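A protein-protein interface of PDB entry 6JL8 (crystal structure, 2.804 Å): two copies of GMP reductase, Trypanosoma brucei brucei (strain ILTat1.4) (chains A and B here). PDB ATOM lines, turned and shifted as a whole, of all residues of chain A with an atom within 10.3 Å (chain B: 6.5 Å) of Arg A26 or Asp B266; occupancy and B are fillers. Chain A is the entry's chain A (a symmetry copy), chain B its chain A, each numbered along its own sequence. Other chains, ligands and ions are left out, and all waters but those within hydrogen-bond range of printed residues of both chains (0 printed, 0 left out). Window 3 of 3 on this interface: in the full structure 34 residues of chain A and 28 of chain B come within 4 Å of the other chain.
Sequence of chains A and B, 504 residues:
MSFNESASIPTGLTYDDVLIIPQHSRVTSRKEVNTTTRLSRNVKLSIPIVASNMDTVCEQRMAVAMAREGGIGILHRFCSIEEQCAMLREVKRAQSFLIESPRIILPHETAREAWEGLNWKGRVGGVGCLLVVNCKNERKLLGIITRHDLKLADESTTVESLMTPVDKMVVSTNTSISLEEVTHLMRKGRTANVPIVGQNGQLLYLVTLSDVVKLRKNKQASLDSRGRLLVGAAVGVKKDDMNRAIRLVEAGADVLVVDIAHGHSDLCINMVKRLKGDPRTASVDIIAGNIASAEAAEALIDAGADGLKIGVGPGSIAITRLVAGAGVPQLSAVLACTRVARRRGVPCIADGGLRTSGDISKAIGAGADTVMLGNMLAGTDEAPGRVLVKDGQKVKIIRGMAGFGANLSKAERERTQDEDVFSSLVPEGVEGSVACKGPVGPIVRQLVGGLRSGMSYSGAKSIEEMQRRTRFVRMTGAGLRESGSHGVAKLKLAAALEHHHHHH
Printed residues of chain B within 4 Å of Ser A25: His B262, His B264, Ser B265 and Asp B266.
Of the printed residues of chain B, Arg A26 touches Asp B266 (3.4 Å).
Of the printed residues of chain B, Val A27 touches Leu B267.
Of the printed residues of chain B, Ser A456 touches His B262.
Of chain A, only His A24 and Ser A25 come within 4 Å of Ser B265.
Asp B266 touches just these residues of chain A: His A24, Ser A25 and Arg A26.
No residue of chain A comes within 4 Å of Ile B269.
No residue of chain A comes within 4 Å of Asn B270.
The nearest residue of chain B that does not touch Arg A26 is Ser B265 (5.5 Å).
The nearest residue of chain A that does not touch Asp B266 is Val A27 (5.3 Å).
The nearest printed residue of chain B that does not touch Ser A25 is Leu B267 (5.0 Å).
O of Asp B266 lies close to ND2 of Asn B270 (3.4 Å).
NE2 of His B262 is in hydrogen-bond range of O of His B264, 3.5 Å away.
N of Gln A23 sits at hydrogen-bond distance from O of Tyr A457.
O of His B262 sits at hydrogen-bond distance from OG of Ser B265, at 3.0 Å.
The backbone carbonyl oxygen (O) of Arg A469 lies close to the side-chain amide oxygen (OE1) of Gln A23 (2.9 Å).
The side-chain hydroxyl of Ser B265 is in hydrogen-bond range of the backbone NH of Cys B268 (3.2 Å).
His B262 touches Pro A22 (CE1 to CB, 3.5 Å).
His B264 touches Gln A23.
His B264 touches His A24 (O to CA, 3.4 Å).
His A24 touches Ser B265 (ND1 to CA, 3.9 Å).
CB of Ser A25 touches NE2 of His B262, at 3.5 Å.
Ser A25 touches Ser B265 (O to CA, 3.4 Å).
Arg A26 touches Asp B266.
Val A27 touches Leu B267 (O to CD1, 3.98 Å).
His B262 touches Tyr A457.
OD1 of Asp B266 lies close to NE2 of His A24 (3.1 Å).
N of Ser A25 is in hydrogen-bond range of O of His B264.
NE2 of His B262 is in hydrogen-bond range of O of Gln A23 (2.8 Å).
N of Asp B266 lies within hydrogen-bond range of O of Ser A25, 3.1 Å away.
NE2 of His B262 sits close to O of Ser A456, at 3.5 Å.
Printed residues of chain B that touch a printed residue of chain A: His B262, His B264, Ser B265, Asp B266 and Leu B267.
Hydrophobic or aromatic side chains of chain A within 4 Å of the printed part of chain B: Pro A22, His A24 and Tyr A457.
Along chain A the printed residues that touch a printed residue of chain B span positions 22 to 457.
Among the printed residues, no Asp or Glu carboxylate lies within 4 Å of a Lys or Arg side-chain nitrogen of the other chain.
No position is printed for both chains.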
ATOM      1  N   PRO A  22      18.682   2.924   3.492  1.00  0.00           N
ATOM      2  CA  PRO A  22      18.983   1.698   2.737  1.00  0.00           C
ATOM      3  C   PRO A  22      18.181   0.519   3.270  1.00  0.00           C
ATOM      4  O   PRO A  22      17.984   0.382   4.473  1.00  0.00           O
ATOM      5  CB  PRO A  22      20.485   1.487   2.960  1.00  0.00           C
ATOM      6  CG  PRO A  22      20.979   2.742   3.499  1.00  0.00           C
ATOM      7  CD  PRO A  22      19.876   3.435   4.185  1.00  0.00           C
ATOM      8  N   GLN A  23      17.730  -0.331   2.348  1.00  0.00           N
ATOM      9  CA  GLN A  23      16.912  -1.506   2.613  1.00  0.00           C
ATOM     10  C   GLN A  23      17.566  -2.690   1.916  1.00  0.00           C
ATOM     11  O   GLN A  23      18.513  -2.525   1.129  1.00  0.00           O
ATOM     12  CB  GLN A  23      15.478  -1.291   2.130  1.00  0.00           C
ATOM     13  CG  GLN A  23      14.744  -0.150   2.831  1.00  0.00           C
ATOM     14  CD  GLN A  23      13.345  -0.570   3.203  1.00  0.00           C
ATOM     15  OE1 GLN A  23      12.456  -0.633   2.335  1.00  0.00           O
ATOM     16  NE2 GLN A  23      13.133  -0.908   4.490  1.00  0.00           N
ATOM     17  N   HIS A  24      17.089  -3.900   2.230  1.00  0.00           N
ATOM     18  CA  HIS A  24      17.761  -5.095   1.724  1.00  0.00           C
ATOM     19  C   HIS A  24      17.619  -5.159   0.209  1.00  0.00           C
ATOM     20  O   HIS A  24      16.499  -5.140  -0.310  1.00  0.00           O
ATOM     21  CB  HIS A  24      17.203  -6.355   2.392  1.00  0.00           C
ATOM     22  CG  HIS A  24      17.793  -7.653   1.904  1.00  0.00           C
ATOM     23  ND1 HIS A  24      18.822  -7.727   0.992  1.00  0.00           N
ATOM     24  CD2 HIS A  24      17.482  -8.937   2.210  1.00  0.00           C
ATOM     25  CE1 HIS A  24      19.118  -8.991   0.750  1.00  0.00           C
ATOM     26  NE2 HIS A  24      18.318  -9.747   1.477  1.00  0.00           N
ATOM     27  N   SER A  25      18.779  -5.206  -0.490  1.00  0.00           N
ATOM     28  CA  SER A  25      18.872  -5.197  -1.948  1.00  0.00           C
ATOM     29  C   SER A  25      19.147  -6.613  -2.457  1.00  0.00           C
ATOM     30  O   SER A  25      20.251  -7.145  -2.287  1.00  0.00           O
ATOM     31  CB  SER A  25      19.979  -4.236  -2.379  1.00  0.00           C
ATOM     32  OG  SER A  25      20.466  -4.473  -3.692  1.00  0.00           O
ATOM     33  N   ARG A  26      18.148  -7.242  -3.065  1.00  0.00           N
ATOM     34  CA  ARG A  26      18.373  -8.548  -3.680  1.00  0.00           C
ATOM     35  C   ARG A  26      18.880  -8.406  -5.117  1.00  0.00           C
ATOM     36  O   ARG A  26      19.001  -9.407  -5.828  1.00  0.00           O
ATOM     37  CB  ARG A  26      17.098  -9.442  -3.594  1.00  0.00           C
ATOM     38  N   VAL A  27      19.239  -7.195  -5.529  1.00  0.00           N
ATOM     39  CA  VAL A  27      19.712  -6.925  -6.887  1.00  0.00           C
ATOM     40  C   VAL A  27      21.163  -7.352  -7.013  1.00  0.00           C
ATOM     41  O   VAL A  27      22.004  -6.957  -6.200  1.00  0.00           O
ATOM     42  CB  VAL A  27      19.547  -5.436  -7.215  1.00  0.00           C
ATOM     43  CG1 VAL A  27      20.561  -4.969  -8.268  1.00  0.00           C
ATOM     44  CG2 VAL A  27      18.127  -5.181  -7.655  1.00  0.00           C
ATOM     45  N   THR A  28      21.462  -8.182  -8.010  1.00  0.00           N
ATOM     46  CA  THR A  28      22.851  -8.475  -8.366  1.00  0.00           C
ATOM     47  C   THR A  28      23.267  -7.695  -9.610  1.00  0.00           C
ATOM     48  O   THR A  28      24.105  -6.790  -9.525  1.00  0.00           O
ATOM     49  CB  THR A  28      23.070  -9.981  -8.570  1.00  0.00           C
ATOM     50  N   SER A  29      22.652  -7.999 -10.756  1.00  0.00           N
ATOM     51  CA  SER A  29      22.946  -7.349 -12.040  1.00  0.00           C
ATOM     52  C   SER A  29      22.520  -5.881 -12.021  1.00  0.00           C
ATOM     53  O   SER A  29      21.343  -5.568 -12.204  1.00  0.00           O
ATOM     54  CB  SER A  29      22.237  -8.102 -13.161  1.00  0.00           C
ATOM     55  N   ARG A  30      23.488  -4.967 -11.851  1.00  0.00           N
ATOM     56  CA  ARG A  30      23.211  -3.531 -11.714  1.00  0.00           C
ATOM     57  C   ARG A  30      22.423  -2.948 -12.890  1.00  0.00           C
ATOM     58  O   ARG A  30      22.026  -1.769 -12.831  1.00  0.00           O
ATOM     59  CB  ARG A  30      24.522  -2.747 -11.531  1.00  0.00           C
ATOM     60  N   GLU A  32      19.724  -5.061 -14.101  1.00  0.00           N
ATOM     61  CA  GLU A  32      18.413  -5.708 -14.083  1.00  0.00           C
ATOM     62  C   GLU A  32      17.367  -4.784 -13.446  1.00  0.00           C
ATOM     63  O   GLU A  32      16.303  -5.236 -12.985  1.00  0.00           O
ATOM     64  CB  GLU A  32      18.483  -7.063 -13.366  1.00  0.00           C
ATOM     65  CG  GLU A  32      18.677  -7.001 -11.852  1.00  0.00           C
ATOM     66  CD  GLU A  32      18.818  -8.372 -11.215  1.00  0.00           C
ATOM     67  OE1 GLU A  32      19.613  -8.506 -10.251  1.00  0.00           O
ATOM     68  OE2 GLU A  32      18.125  -9.310 -11.676  1.00  0.00           O
ATOM     69  N   VAL A  33      17.689  -3.490 -13.409  1.00  0.00           N
ATOM     70  CA  VAL A  33      16.844  -2.444 -12.854  1.00  0.00           C
ATOM     71  C   VAL A  33      16.139  -1.764 -14.008  1.00  0.00           C
ATOM     72  O   VAL A  33      16.783  -1.123 -14.855  1.00  0.00           O
ATOM     73  CB  VAL A  33      17.666  -1.424 -12.059  1.00  0.00           C
ATOM     74  CG1 VAL A  33      16.759  -0.436 -11.429  1.00  0.00           C
ATOM     75  CG2 VAL A  33      18.537  -2.112 -11.029  1.00  0.00           C
ATOM     76  N   MET A 455      17.608   3.412  -6.464  1.00  0.00           N
ATOM     77  CA  MET A 455      16.687   2.286  -6.407  1.00  0.00           C
ATOM     78  C   MET A 455      17.326   1.084  -5.721  1.00  0.00           C
ATOM     79  O   MET A 455      16.647   0.333  -4.987  1.00  0.00           O
ATOM     80  CB  MET A 455      16.223   1.923  -7.827  1.00  0.00           C
ATOM     81  CG  MET A 455      15.616   3.093  -8.587  1.00  0.00           C
ATOM     82  SD  MET A 455      15.286   2.777 -10.326  1.00  0.00           S
ATOM     83  CE  MET A 455      14.001   1.562 -10.278  1.00  0.00           C
ATOM     84  N   SER A 456      18.632   0.896  -5.925  1.00  0.00           N
ATOM     85  CA  SER A 456      19.276  -0.269  -5.332  1.00  0.00           C
ATOM     86  C   SER A 456      19.366  -0.122  -3.823  1.00  0.00           C
ATOM     87  O   SER A 456      19.356  -1.127  -3.107  1.00  0.00           O
ATOM     88  CB  SER A 456      20.656  -0.511  -5.974  1.00  0.00           C
ATOM     89  OG  SER A 456      21.722   0.126  -5.274  1.00  0.00           O
ATOM     90  N   TYR A 457      19.440   1.119  -3.322  1.00  0.00           N
ATOM     91  CA  TYR A 457      19.338   1.323  -1.892  1.00  0.00           C
ATOM     92  C   TYR A 457      17.931   1.002  -1.378  1.00  0.00           C
ATOM     93  O   TYR A 457      17.767   0.513  -0.241  1.00  0.00           O
ATOM     94  CB  TYR A 457      19.738   2.739  -1.568  1.00  0.00           C
ATOM     95  CG  TYR A 457      21.233   2.865  -1.495  1.00  0.00           C
ATOM     96  CD1 TYR A 457      21.932   2.342  -0.419  1.00  0.00           C
ATOM     97  CD2 TYR A 457      21.961   3.474  -2.526  1.00  0.00           C
ATOM     98  CE1 TYR A 457      23.299   2.422  -0.362  1.00  0.00           C
ATOM     99  CE2 TYR A 457      23.336   3.572  -2.464  1.00  0.00           C
ATOM    100  CZ  TYR A 457      23.992   3.040  -1.393  1.00  0.00           C
ATOM    101  OH  TYR A 457      25.341   3.126  -1.333  1.00  0.00           O
ATOM    102  N   SER A 458      16.912   1.247  -2.198  1.00  0.00           N
ATOM    103  CA  SER A 458      15.559   0.948  -1.778  1.00  0.00           C
ATOM    104  C   SER A 458      15.204  -0.509  -1.994  1.00  0.00           C
ATOM    105  O   SER A 458      14.083  -0.916  -1.672  1.00  0.00           O
ATOM    106  CB  SER A 458      14.578   1.855  -2.527  1.00  0.00           C
ATOM    107  OG  SER A 458      14.585   3.149  -1.969  1.00  0.00           O
ATOM    108  N   GLY A 459      16.103  -1.294  -2.576  1.00  0.00           N
ATOM    109  CA  GLY A 459      15.742  -2.675  -2.827  1.00  0.00           C
ATOM    110  C   GLY A 459      14.686  -2.764  -3.906  1.00  0.00           C
ATOM    111  O   GLY A 459      13.692  -3.492  -3.770  1.00  0.00           O
ATOM    112  N   ALA A 460      14.908  -2.033  -5.001  1.00  0.00           N
ATOM    113  CA  ALA A 460      13.858  -1.791  -5.979  1.00  0.00           C
ATOM    114  C   ALA A 460      14.381  -2.175  -7.340  1.00  0.00           C
ATOM    115  O   ALA A 460      15.381  -1.612  -7.800  1.00  0.00           O
ATOM    116  CB  ALA A 460      13.418  -0.325  -5.977  1.00  0.00           C
ATOM    117  N   LYS A 461      13.699  -3.115  -7.986  1.00  0.00           N
ATOM    118  CA  LYS A 461      14.075  -3.542  -9.324  1.00  0.00           C
ATOM    119  C   LYS A 461      13.214  -2.880 -10.416  1.00  0.00           C
ATOM    120  O   LYS A 461      13.515  -3.033 -11.600  1.00  0.00           O
ATOM    121  CB  LYS A 461      14.056  -5.083  -9.390  1.00  0.00           C
ATOM    122  N   GLU A 465       8.439  -0.283  -7.807  1.00  0.00           N
ATOM    123  CA  GLU A 465       9.028  -0.777  -6.570  1.00  0.00           C
ATOM    124  C   GLU A 465       9.672   0.362  -5.785  1.00  0.00           C
ATOM    125  O   GLU A 465       9.455   0.498  -4.576  1.00  0.00           O
ATOM    126  CB  GLU A 465      10.042  -1.874  -6.876  1.00  0.00           C
ATOM    127  CG  GLU A 465       9.497  -3.290  -7.000  1.00  0.00           C
ATOM    128  CD  GLU A 465      10.627  -4.273  -7.315  1.00  0.00           C
ATOM    129  OE1 GLU A 465      11.614  -4.346  -6.526  1.00  0.00           O
ATOM    130  OE2 GLU A 465      10.559  -4.948  -8.372  1.00  0.00           O
ATOM    131  N   ARG A 469       8.533   0.980  -1.919  1.00  0.00           N
ATOM    132  CA  ARG A 469       9.424   0.444  -0.915  1.00  0.00           C
ATOM    133  C   ARG A 469      10.231   1.496  -0.180  1.00  0.00           C
ATOM    134  O   ARG A 469      10.665   1.250   0.954  1.00  0.00           O
ATOM    135  CB  ARG A 469      10.366  -0.554  -1.561  1.00  0.00           C
ATOM    136  CG  ARG A 469       9.617  -1.603  -2.283  1.00  0.00           C
ATOM    137  CD  ARG A 469      10.431  -2.867  -2.363  1.00  0.00           C
ATOM    138  NE  ARG A 469       9.880  -3.772  -3.374  1.00  0.00           N
ATOM    139  CZ  ARG A 469      10.343  -4.995  -3.573  1.00  0.00           C
ATOM    140  NH1 ARG A 469      11.344  -5.426  -2.826  1.00  0.00           N
ATOM    141  NH2 ARG A 469       9.806  -5.786  -4.491  1.00  0.00           N
ATOM    142  N   HIS B 262      26.880  -0.652  -0.177  1.00  0.00           N
ATOM    143  CA  HIS B 262      25.538  -1.073   0.297  1.00  0.00           C
ATOM    144  C   HIS B 262      25.635  -2.499   0.820  1.00  0.00           C
ATOM    145  O   HIS B 262      25.261  -3.452   0.141  1.00  0.00           O
ATOM    146  CB  HIS B 262      24.457  -0.936  -0.793  1.00  0.00           C
ATOM    147  CG  HIS B 262      23.062  -1.223  -0.324  1.00  0.00           C
ATOM    148  ND1 HIS B 262      22.657  -1.032   0.978  1.00  0.00           N
ATOM    149  CD2 HIS B 262      21.976  -1.703  -0.986  1.00  0.00           C
ATOM    150  CE1 HIS B 262      21.381  -1.366   1.096  1.00  0.00           C
ATOM    151  NE2 HIS B 262      20.949  -1.793  -0.077  1.00  0.00           N
ATOM    152  N   GLY B 263      26.103  -2.636   2.062  1.00  0.00           N
ATOM    153  CA  GLY B 263      26.321  -3.945   2.640  1.00  0.00           C
ATOM    154  C   GLY B 263      25.059  -4.712   2.960  1.00  0.00           C
ATOM    155  O   GLY B 263      25.109  -5.939   3.091  1.00  0.00           O
ATOM    156  N   HIS B 264      23.924  -4.036   3.104  1.00  0.00           N
ATOM    157  CA  HIS B 264      22.688  -4.775   3.329  1.00  0.00           C
ATOM    158  C   HIS B 264      22.172  -5.316   2.004  1.00  0.00           C
ATOM    159  O   HIS B 264      21.135  -4.900   1.484  1.00  0.00           O
ATOM    160  CB  HIS B 264      21.629  -3.924   3.988  1.00  0.00           C
ATOM    161  CG  HIS B 264      20.503  -4.736   4.543  1.00  0.00           C
ATOM    162  ND1 HIS B 264      19.369  -4.175   5.088  1.00  0.00           N
ATOM    163  CD2 HIS B 264      20.348  -6.074   4.647  1.00  0.00           C
ATOM    164  CE1 HIS B 264      18.560  -5.133   5.494  1.00  0.00           C
ATOM    165  NE2 HIS B 264      19.135  -6.293   5.248  1.00  0.00           N
ATOM    166  N   SER B 265      22.890  -6.296   1.475  1.00  0.00           N
ATOM    167  CA  SER B 265      22.544  -6.813   0.159  1.00  0.00           C
ATOM    168  C   SER B 265      22.927  -8.286   0.062  1.00  0.00           C
ATOM    169  O   SER B 265      23.819  -8.763   0.775  1.00  0.00           O
ATOM    170  CB  SER B 265      23.258  -5.988  -0.917  1.00  0.00           C
ATOM    171  OG  SER B 265      24.648  -6.175  -0.818  1.00  0.00           O
ATOM    172  N   ASP B 266      22.258  -9.009  -0.844  1.00  0.00           N
ATOM    173  CA  ASP B 266      22.671 -10.396  -1.089  1.00  0.00           C
ATOM    174  C   ASP B 266      24.137 -10.472  -1.521  1.00  0.00           C
ATOM    175  O   ASP B 266      24.879 -11.340  -1.060  1.00  0.00           O
ATOM    176  CB  ASP B 266      21.781 -11.060  -2.134  1.00  0.00           C
ATOM    177  CG  ASP B 266      20.385 -11.341  -1.624  1.00  0.00           C
ATOM    178  OD1 ASP B 266      20.199 -11.347  -0.375  1.00  0.00           O
ATOM    179  OD2 ASP B 266      19.485 -11.563  -2.487  1.00  0.00           O
ATOM    180  N   LEU B 267      24.572  -9.570  -2.398  1.00  0.00           N
ATOM    181  CA  LEU B 267      25.981  -9.499  -2.752  1.00  0.00           C
ATOM    182  C   LEU B 267      26.877  -9.575  -1.518  1.00  0.00           C
ATOM    183  O   LEU B 267      27.722 -10.470  -1.389  1.00  0.00           O
ATOM    184  CB  LEU B 267      26.238  -8.194  -3.497  1.00  0.00           C
ATOM    185  CG  LEU B 267      25.737  -8.066  -4.923  1.00  0.00           C
ATOM    186  CD1 LEU B 267      25.875  -6.611  -5.353  1.00  0.00           C
ATOM    187  CD2 LEU B 267      26.587  -8.973  -5.737  1.00  0.00           C
ATOM    188  N   CYS B 268      26.701  -8.623  -0.595  1.00  0.00           N
ATOM    189  CA  CYS B 268      27.512  -8.598   0.615  1.00  0.00           C
ATOM    190  C   CYS B 268      27.342  -9.872   1.428  1.00  0.00           C
ATOM    191  O   CYS B 268      28.338 -10.542   1.738  1.00  0.00           O
ATOM    192  CB  CYS B 268      27.160  -7.371   1.461  1.00  0.00           C
ATOM    193  SG  CYS B 268      28.158  -7.226   2.999  1.00  0.00           S
ATOM    194  N   ILE B 269      26.090 -10.202   1.798  1.00  0.00           N
ATOM    195  CA  ILE B 269      25.836 -11.421   2.565  1.00  0.00           C
ATOM    196  C   ILE B 269      26.540 -12.609   1.916  1.00  0.00           C
ATOM    197  O   ILE B 269      27.299 -13.349   2.558  1.00  0.00           O
ATOM    198  CB  ILE B 269      24.321 -11.688   2.696  1.00  0.00           C
ATOM    199  CG1 ILE B 269      23.650 -10.747   3.677  1.00  0.00           C
ATOM    200  CG2 ILE B 269      24.097 -13.093   3.115  1.00  0.00           C
ATOM    201  CD1 ILE B 269      22.340 -10.219   3.151  1.00  0.00           C
ATOM    202  N   ASN B 270      26.301 -12.802   0.626  1.00  0.00           N
ATOM    203  CA  ASN B 270      26.817 -13.993  -0.021  1.00  0.00           C
ATOM    204  C   ASN B 270      28.339 -14.023   0.019  1.00  0.00           C
ATOM    205  O   ASN B 270      28.928 -15.098   0.180  1.00  0.00           O
ATOM    206  CB  ASN B 270      26.279 -14.061  -1.454  1.00  0.00           C
ATOM    207  CG  ASN B 270      24.835 -14.544  -1.516  1.00  0.00           C
ATOM    208  OD1 ASN B 270      24.299 -15.136  -0.563  1.00  0.00           O
ATOM    209  ND2 ASN B 270      24.195 -14.281  -2.639  1.00  0.00           N
ATOM    210  N   MET B 271      28.983 -12.854  -0.084  1.00  0.00           N
ATOM    211  CA  MET B 271      30.427 -12.757   0.101  1.00  0.00           C
ATOM    212  C   MET B 271      30.849 -13.237   1.486  1.00  0.00           C
ATOM    213  O   MET B 271      31.796 -14.021   1.620  1.00  0.00           O
ATOM    214  CB  MET B 271      30.873 -11.297  -0.120  1.00  0.00           C
ATOM    215  CG  MET B 271      32.365 -11.060  -0.138  1.00  0.00           C
ATOM    216  SD  MET B 271      33.019 -12.323  -1.223  1.00  0.00           S
ATOM    217  CE  MET B 271      34.673 -11.749  -1.634  1.00  0.00           C
